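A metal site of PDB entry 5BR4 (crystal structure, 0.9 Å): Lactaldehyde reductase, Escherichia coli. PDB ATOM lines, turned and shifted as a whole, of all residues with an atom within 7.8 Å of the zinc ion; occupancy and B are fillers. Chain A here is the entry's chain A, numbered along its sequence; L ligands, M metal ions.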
ATOM      1  N   GLY A 143      25.898  -7.097 -25.354  1.00  0.00           N
ATOM      2  CA  GLY A 143      25.409  -7.863 -26.467  1.00  0.00           C
ATOM      3  C   GLY A 143      23.916  -8.048 -26.458  1.00  0.00           C
ATOM      4  O   GLY A 143      23.225  -7.659 -25.520  1.00  0.00           O
ATOM      5  N   THR A 144      23.408  -8.651 -27.527  1.00  0.00           N
ATOM      6  CA  THR A 144      21.978  -8.759 -27.799  1.00  0.00           C
ATOM      7  C   THR A 144      21.324 -10.028 -27.276  1.00  0.00           C
ATOM      8  O   THR A 144      20.110 -10.100 -27.203  1.00  0.00           O
ATOM      9  CB  THR A 144      21.742  -8.707 -29.320  1.00  0.00           C
ATOM     10  OG1 THR A 144      22.331  -9.853 -29.967  1.00  0.00           O
ATOM     11  CG2 THR A 144      22.225  -7.371 -29.902  1.00  0.00           C
ATOM     12  N   ALA A 145      22.157 -11.040 -26.973  1.00  0.00           N
ATOM     13  CA  ALA A 145      21.684 -12.365 -26.629  1.00  0.00           C
ATOM     14  C   ALA A 145      20.904 -13.007 -27.777  1.00  0.00           C
ATOM     15  O   ALA A 145      20.176 -13.986 -27.584  1.00  0.00           O
ATOM     16  CB  ALA A 145      20.906 -12.417 -25.329  1.00  0.00           C
ATOM     17  N   ALA A 192      28.058   0.708 -25.244  1.00  0.00           N
ATOM     18  CA  ALA A 192      26.663   0.770 -25.730  1.00  0.00           C
ATOM     19  C   ALA A 192      26.013  -0.569 -25.696  1.00  0.00           C
ATOM     20  O   ALA A 192      24.854  -0.726 -25.315  1.00  0.00           O
ATOM     21  CB  ALA A 192      26.656   1.376 -27.134  1.00  0.00           C
ATOM     22  N   THR A 193      26.722  -1.612 -26.224  1.00  0.00           N
ATOM     23  CA  THR A 193      26.147  -2.970 -26.219  1.00  0.00           C
ATOM     24  C   THR A 193      25.973  -3.485 -24.807  1.00  0.00           C
ATOM     25  O   THR A 193      25.029  -4.271 -24.546  1.00  0.00           O
ATOM     26  CB  THR A 193      26.997  -3.929 -27.052  1.00  0.00           C
ATOM     27  OG1 THR A 193      28.321  -4.039 -26.525  1.00  0.00           O
ATOM     28  CG2 THR A 193      27.014  -3.549 -28.539  1.00  0.00           C
ATOM     29  N   VAL A 195      25.289  -1.537 -22.002  1.00  0.00           N
ATOM     30  CA  VAL A 195      24.098  -0.935 -21.458  1.00  0.00           C
ATOM     31  C   VAL A 195      22.828  -1.464 -22.145  1.00  0.00           C
ATOM     32  O   VAL A 195      21.765  -1.607 -21.510  1.00  0.00           O
ATOM     33  CB  VAL A 195      24.153   0.614 -21.437  1.00  0.00           C
ATOM     34  CG1 VAL A 195      22.872   1.179 -20.898  1.00  0.00           C
ATOM     35  CG2 VAL A 195      25.334   1.106 -20.608  1.00  0.00           C
ATOM     36  N   ASP A 196      22.912  -1.842 -23.403  1.00  0.00           N
ATOM     37  CA  ASP A 196      21.817  -2.552 -24.048  1.00  0.00           C
ATOM     38  C   ASP A 196      21.528  -3.909 -23.364  1.00  0.00           C
ATOM     39  O   ASP A 196      20.369  -4.247 -23.101  1.00  0.00           O
ATOM     40  CB  ASP A 196      22.134  -2.767 -25.526  1.00  0.00           C
ATOM     41  CG  ASP A 196      21.028  -3.441 -26.234  1.00  0.00           C
ATOM     42  OD1 ASP A 196      19.820  -2.995 -26.059  1.00  0.00           O
ATOM     43  OD2 ASP A 196      21.258  -4.382 -27.014  1.00  0.00           O
ATOM     44  N   ALA A 197      22.600  -4.659 -23.019  1.00  0.00           N
ATOM     45  CA  ALA A 197      22.382  -5.888 -22.259  1.00  0.00           C
ATOM     46  C   ALA A 197      21.698  -5.593 -20.938  1.00  0.00           C
ATOM     47  O   ALA A 197      20.749  -6.311 -20.541  1.00  0.00           O
ATOM     48  CB  ALA A 197      23.708  -6.599 -22.046  1.00  0.00           C
ATOM     49  N   LEU A 198      22.114  -4.533 -20.256  1.00  0.00           N
ATOM     50  CA  LEU A 198      21.454  -4.118 -19.041  1.00  0.00           C
ATOM     51  C   LEU A 198      19.996  -3.780 -19.261  1.00  0.00           C
ATOM     52  O   LEU A 198      19.119  -4.130 -18.468  1.00  0.00           O
ATOM     53  CB  LEU A 198      22.205  -2.938 -18.407  1.00  0.00           C
ATOM     54  CG  LEU A 198      21.648  -2.487 -17.051  1.00  0.00           C
ATOM     55  CD1 LEU A 198      21.855  -3.514 -15.950  1.00  0.00           C
ATOM     56  CD2 LEU A 198      22.269  -1.134 -16.633  1.00  0.00           C
ATOM     57  N   THR A 199      19.727  -3.108 -20.399  1.00  0.00           N
ATOM     58  CA  THR A 199      18.332  -2.770 -20.772  1.00  0.00           C
ATOM     59  C   THR A 199      17.497  -4.046 -20.942  1.00  0.00           C
ATOM     60  O   THR A 199      16.333  -4.113 -20.503  1.00  0.00           O
ATOM     61  CB  THR A 199      18.335  -1.957 -22.087  1.00  0.00           C
ATOM     62  OG1 THR A 199      19.092  -0.745 -21.903  1.00  0.00           O
ATOM     63  CG2 THR A 199      16.904  -1.542 -22.420  1.00  0.00           C
ATOM     64  N   HIS A 200      18.066  -5.059 -21.623  1.00  0.00           N
ATOM     65  CA  HIS A 200      17.316  -6.296 -21.765  1.00  0.00           C
ATOM     66  C   HIS A 200      16.936  -6.876 -20.421  1.00  0.00           C
ATOM     67  O   HIS A 200      15.816  -7.333 -20.205  1.00  0.00           O
ATOM     68  CB  HIS A 200      18.169  -7.348 -22.495  1.00  0.00           C
ATOM     69  CG  HIS A 200      18.511  -6.964 -23.889  1.00  0.00           C
ATOM     70  ND1 HIS A 200      19.733  -7.256 -24.440  1.00  0.00           N
ATOM     71  CD2 HIS A 200      17.902  -6.168 -24.771  1.00  0.00           C
ATOM     72  CE1 HIS A 200      19.856  -6.630 -25.603  1.00  0.00           C
ATOM     73  NE2 HIS A 200      18.737  -5.965 -25.856  1.00  0.00           N
ATOM     74  N   GLU A 203      14.370  -4.341 -18.565  1.00  0.00           N
ATOM     75  CA  GLU A 203      13.030  -4.428 -19.151  1.00  0.00           C
ATOM     76  C   GLU A 203      12.401  -5.796 -18.948  1.00  0.00           C
ATOM     77  O   GLU A 203      11.219  -5.921 -18.677  1.00  0.00           O
ATOM     78  CB  GLU A 203      13.031  -4.082 -20.640  1.00  0.00           C
ATOM     79  CG  GLU A 203      13.450  -2.650 -20.927  1.00  0.00           C
ATOM     80  CD  GLU A 203      12.735  -2.123 -22.204  1.00  0.00           C
ATOM     81  OE1 GLU A 203      11.712  -1.402 -22.012  1.00  0.00           O
ATOM     82  OE2 GLU A 203      13.127  -2.493 -23.335  1.00  0.00           O
ATOM     83  N   PHE A 254      14.448 -12.753 -21.414  1.00  0.00           N
ATOM     84  CA  PHE A 254      13.581 -11.821 -22.129  1.00  0.00           C
ATOM     85  C   PHE A 254      13.034 -12.447 -23.381  1.00  0.00           C
ATOM     86  O   PHE A 254      11.930 -12.046 -23.851  1.00  0.00           O
ATOM     87  CB  PHE A 254      14.182 -10.449 -22.398  1.00  0.00           C
ATOM     88  CG  PHE A 254      15.210 -10.382 -23.532  1.00  0.00           C
ATOM     89  CD1 PHE A 254      14.798 -10.271 -24.850  1.00  0.00           C
ATOM     90  CD2 PHE A 254      16.550 -10.341 -23.293  1.00  0.00           C
ATOM     91  CE1 PHE A 254      15.740 -10.148 -25.871  1.00  0.00           C
ATOM     92  CE2 PHE A 254      17.485 -10.248 -24.306  1.00  0.00           C
ATOM     93  CZ  PHE A 254      17.044 -10.140 -25.587  1.00  0.00           C
ATOM     94  N   LEU A 259      10.003  -7.402 -23.413  1.00  0.00           N
ATOM     95  CA  LEU A 259      10.791  -6.222 -23.058  1.00  0.00           C
ATOM     96  C   LEU A 259       9.835  -5.091 -22.708  1.00  0.00           C
ATOM     97  O   LEU A 259       8.832  -5.275 -21.954  1.00  0.00           O
ATOM     98  CB  LEU A 259      11.803  -5.881 -24.165  1.00  0.00           C
ATOM     99  CG  LEU A 259      12.936  -6.922 -24.333  1.00  0.00           C
ATOM    100  CD1 LEU A 259      13.713  -6.611 -25.583  1.00  0.00           C
ATOM    101  CD2 LEU A 259      13.831  -6.973 -23.132  1.00  0.00           C
ATOM    102  N   VAL A 262      11.539   0.862 -23.731  1.00  0.00           N
ATOM    103  CA  VAL A 262      12.870   1.286 -24.189  1.00  0.00           C
ATOM    104  C   VAL A 262      13.121   0.753 -25.595  1.00  0.00           C
ATOM    105  O   VAL A 262      13.427   1.489 -26.540  1.00  0.00           O
ATOM    106  CB  VAL A 262      14.007   0.865 -23.250  1.00  0.00           C
ATOM    107  CG1 VAL A 262      15.319   1.500 -23.721  1.00  0.00           C
ATOM    108  CG2 VAL A 262      13.736   1.244 -21.786  1.00  0.00           C
ATOM    109  N   HIS A 263      12.948  -0.563 -25.738  1.00  0.00           N
ATOM    110  CA  HIS A 263      13.141  -1.187 -27.048  1.00  0.00           C
ATOM    111  C   HIS A 263      12.154  -0.691 -28.041  1.00  0.00           C
ATOM    112  O   HIS A 263      12.470  -0.554 -29.239  1.00  0.00           O
ATOM    113  CB  HIS A 263      13.166  -2.718 -26.892  1.00  0.00           C
ATOM    114  CG  HIS A 263      14.529  -3.208 -26.500  1.00  0.00           C
ATOM    115  ND1 HIS A 263      15.067  -3.003 -25.246  1.00  0.00           N
ATOM    116  CD2 HIS A 263      15.540  -3.681 -27.257  1.00  0.00           C
ATOM    117  CE1 HIS A 263      16.379  -3.346 -25.328  1.00  0.00           C
ATOM    118  NE2 HIS A 263      16.687  -3.761 -26.495  1.00  0.00           N
ATOM    119  N   ALA A 266      13.434   2.599 -29.249  1.00  0.00           N
ATOM    120  CA  ALA A 266      14.685   2.517 -29.994  1.00  0.00           C
ATOM    121  C   ALA A 266      14.468   2.009 -31.427  1.00  0.00           C
ATOM    122  O   ALA A 266      15.135   2.476 -32.353  1.00  0.00           O
ATOM    123  CB  ALA A 266      15.674   1.643 -29.262  1.00  0.00           C
ATOM    124  N   HIS A 267      13.499   1.081 -31.629  1.00  0.00           N
ATOM    125  CA  HIS A 267      13.302   0.546 -32.981  1.00  0.00           C
ATOM    126  C   HIS A 267      13.093   1.622 -34.030  1.00  0.00           C
ATOM    127  O   HIS A 267      13.739   1.559 -35.101  1.00  0.00           O
ATOM    128  CB  HIS A 267      12.141  -0.445 -33.019  1.00  0.00           C
ATOM    129  CG  HIS A 267      12.483  -1.801 -32.522  1.00  0.00           C
ATOM    130  ND1 HIS A 267      11.543  -2.710 -32.089  1.00  0.00           N
ATOM    131  CD2 HIS A 267      13.672  -2.440 -32.381  1.00  0.00           C
ATOM    132  CE1 HIS A 267      12.109  -3.787 -31.661  1.00  0.00           C
ATOM    133  NE2 HIS A 267      13.405  -3.687 -31.857  1.00  0.00           N
ATOM    134  N   HIS A 277      21.563   0.066 -32.416  1.00  0.00           N
ATOM    135  CA  HIS A 277      20.628  -0.431 -31.427  1.00  0.00           C
ATOM    136  C   HIS A 277      21.092  -0.162 -30.004  1.00  0.00           C
ATOM    137  O   HIS A 277      20.337   0.244 -29.145  1.00  0.00           O
ATOM    138  CB  HIS A 277      20.464  -1.918 -31.669  1.00  0.00           C
ATOM    139  CG  HIS A 277      19.630  -2.624 -30.661  1.00  0.00           C
ATOM    140  ND1 HIS A 277      18.282  -2.689 -30.737  1.00  0.00           N
ATOM    141  CD2 HIS A 277      19.959  -3.336 -29.552  1.00  0.00           C
ATOM    142  CE1 HIS A 277      17.825  -3.349 -29.697  1.00  0.00           C
ATOM    143  NE2 HIS A 277      18.795  -3.815 -28.946  1.00  0.00           N
ATOM    144  N   GLY A 278      22.352  -0.527 -29.756  1.00  0.00           N
ATOM    145  CA  GLY A 278      22.843  -0.450 -28.343  1.00  0.00           C
ATOM    146  C   GLY A 278      22.790   0.950 -27.836  1.00  0.00           C
ATOM    147  O   GLY A 278      22.298   1.220 -26.715  1.00  0.00           O
ATOM    148  N   ASN A 281      19.134   2.319 -27.223  1.00  0.00           N
ATOM    149  CA  ASN A 281      18.566   1.812 -25.956  1.00  0.00           C
ATOM    150  C   ASN A 281      19.231   2.402 -24.756  1.00  0.00           C
ATOM    151  O   ASN A 281      18.549   2.780 -23.773  1.00  0.00           O
ATOM    152  CB  ASN A 281      18.640   0.262 -25.954  1.00  0.00           C
ATOM    153  CG  ASN A 281      17.493  -0.319 -26.730  1.00  0.00           C
ATOM    154  OD1 ASN A 281      16.358  -0.391 -26.285  1.00  0.00           O
ATOM    155  ND2 ASN A 281      17.747  -0.709 -28.016  1.00  0.00           N
ATOM    156  N   ALA A 282      20.546   2.553 -24.791  1.00  0.00           N
ATOM    157  CA  ALA A 282      21.278   3.068 -23.631  1.00  0.00           C
ATOM    158  C   ALA A 282      20.806   4.474 -23.304  1.00  0.00           C
ATOM    159  O   ALA A 282      20.629   4.835 -22.115  1.00  0.00           O
ATOM    160  CB  ALA A 282      22.783   3.035 -23.903  1.00  0.00           C
HETATM  161  P1  LIG L   1      25.676  -5.137 -34.641  1.00  0.00           P
HETATM  162  O1  LIG L   1      25.698  -6.603 -34.909  1.00  0.00           O
HETATM  163  O2  LIG L   1      24.767  -4.303 -35.449  1.00  0.00           O
HETATM  164  O3  LIG L   1      27.175  -4.619 -34.822  1.00  0.00           O
HETATM  165  C1  LIG L   1      27.478  -3.226 -34.686  1.00  0.00           C
HETATM  166  C2  LIG L   1      28.840  -2.952 -35.184  1.00  0.00           C
HETATM  167  O4  LIG L   1      29.853  -3.512 -34.327  1.00  0.00           O
HETATM  168  C3  LIG L   1      29.127  -3.506 -36.585  1.00  0.00           C
HETATM  169  O5  LIG L   1      29.835  -2.576 -37.380  1.00  0.00           O
HETATM  170  C4  LIG L   1      29.995  -4.719 -36.285  1.00  0.00           C
HETATM  171  O6  LIG L   1      30.875  -5.157 -37.333  1.00  0.00           O
HETATM  172  C5  LIG L   1      30.748  -4.248 -35.068  1.00  0.00           C
HETATM  173  N1  LIG L   1      31.298  -5.332 -34.270  1.00  0.00           N
HETATM  174  C6  LIG L   1      30.595  -6.379 -33.758  1.00  0.00           C
HETATM  175  N2  LIG L   1      31.354  -7.215 -33.083  1.00  0.00           N
HETATM  176  C7  LIG L   1      32.638  -6.659 -33.146  1.00  0.00           C
HETATM  177  C8  LIG L   1      33.867  -7.092 -32.608  1.00  0.00           C
HETATM  178  N3  LIG L   1      34.023  -8.185 -31.869  1.00  0.00           N
HETATM  179  N4  LIG L   1      34.977  -6.381 -32.989  1.00  0.00           N
HETATM  180  C9  LIG L   1      34.811  -5.244 -33.687  1.00  0.00           C
HETATM  181  N5  LIG L   1      33.653  -4.717 -34.127  1.00  0.00           N
HETATM  182  C10 LIG L   1      32.592  -5.509 -33.857  1.00  0.00           C
HETATM  183  O7  LIG L   1      25.420  -4.742 -33.089  1.00  0.00           O
HETATM  184  P2  LIG L   1      24.509  -5.464 -31.977  1.00  0.00           P
HETATM  185  O8  LIG L   1      25.163  -6.699 -31.518  1.00  0.00           O
HETATM  186  O9  LIG L   1      24.149  -4.391 -30.993  1.00  0.00           O
HETATM  187  O10 LIG L   1      23.207  -5.939 -32.802  1.00  0.00           O
HETATM  188  C11 LIG L   1      22.129  -4.976 -33.077  1.00  0.00           C
HETATM  189  C12 LIG L   1      21.025  -5.707 -33.794  1.00  0.00           C
HETATM  190  O11 LIG L   1      20.533  -6.771 -32.963  1.00  0.00           O
HETATM  191  C13 LIG L   1      19.832  -4.807 -34.070  1.00  0.00           C
HETATM  192  O12 LIG L   1      19.376  -4.863 -35.433  1.00  0.00           O
HETATM  193  C14 LIG L   1      18.774  -5.281 -33.069  1.00  0.00           C
HETATM  194  O13 LIG L   1      17.413  -5.000 -33.510  1.00  0.00           O
HETATM  195  C15 LIG L   1      19.078  -6.752 -32.947  1.00  0.00           C
HETATM  196  N6  LIG L   1      18.628  -7.422 -31.752  1.00  0.00           N
HETATM  197  C16 LIG L   1      18.076  -8.674 -31.857  1.00  0.00           C
HETATM  198  C17 LIG L   1      17.666  -9.360 -30.722  1.00  0.00           C
HETATM  199  C18 LIG L   1      17.059 -10.720 -30.865  1.00  0.00           C
HETATM  200  O14 LIG L   1      16.385 -11.171 -29.938  1.00  0.00           O
HETATM  201  N7  LIG L   1      17.318 -11.426 -31.967  1.00  0.00           N
HETATM  202  C19 LIG L   1      17.786  -8.751 -29.428  1.00  0.00           C
HETATM  203  C20 LIG L   1      18.380  -7.490 -29.363  1.00  0.00           C
HETATM  204  C21 LIG L   1      18.799  -6.851 -30.489  1.00  0.00           C
HETATM  205 ZN    ZN M   1      18.606  -4.268 -27.004  1.00  0.00          ZN
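O of His 277 is in hydrogen-bond range of ND2 of Asn 281, 3.0 Å away.
The side-chain amide oxygen of Asn 281 is in hydrogen-bond range of a ring nitrogen (ND1) of His 263 (3.1 Å).
A ring nitrogen (ND1) of His 263 sits at hydrogen-bond distance from the side-chain carboxylate (OE2) of Glu 203, 2.8 Å away.
The side-chain amide oxygen of Asn 281 lies close to the backbone carbonyl oxygen of Val 262 (3.5 Å).
Residues that only touch the zinc ion: Asn 281 (3.8 Å).
Within 4 Å of the zinc ion: Asp 196, His 200, His 263, His 277 and Asn 281.
The nearest printed residue that does not touch the zinc ion is Thr 199 (5.4 Å).
The zinc ion is bound by OD1 of Asp 196, NE2 of His 277, NE2 of His 263 and NE2 of His 200.
Slightly farther from the zinc ion lies OD2 of Asp 196 (2.7 Å).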
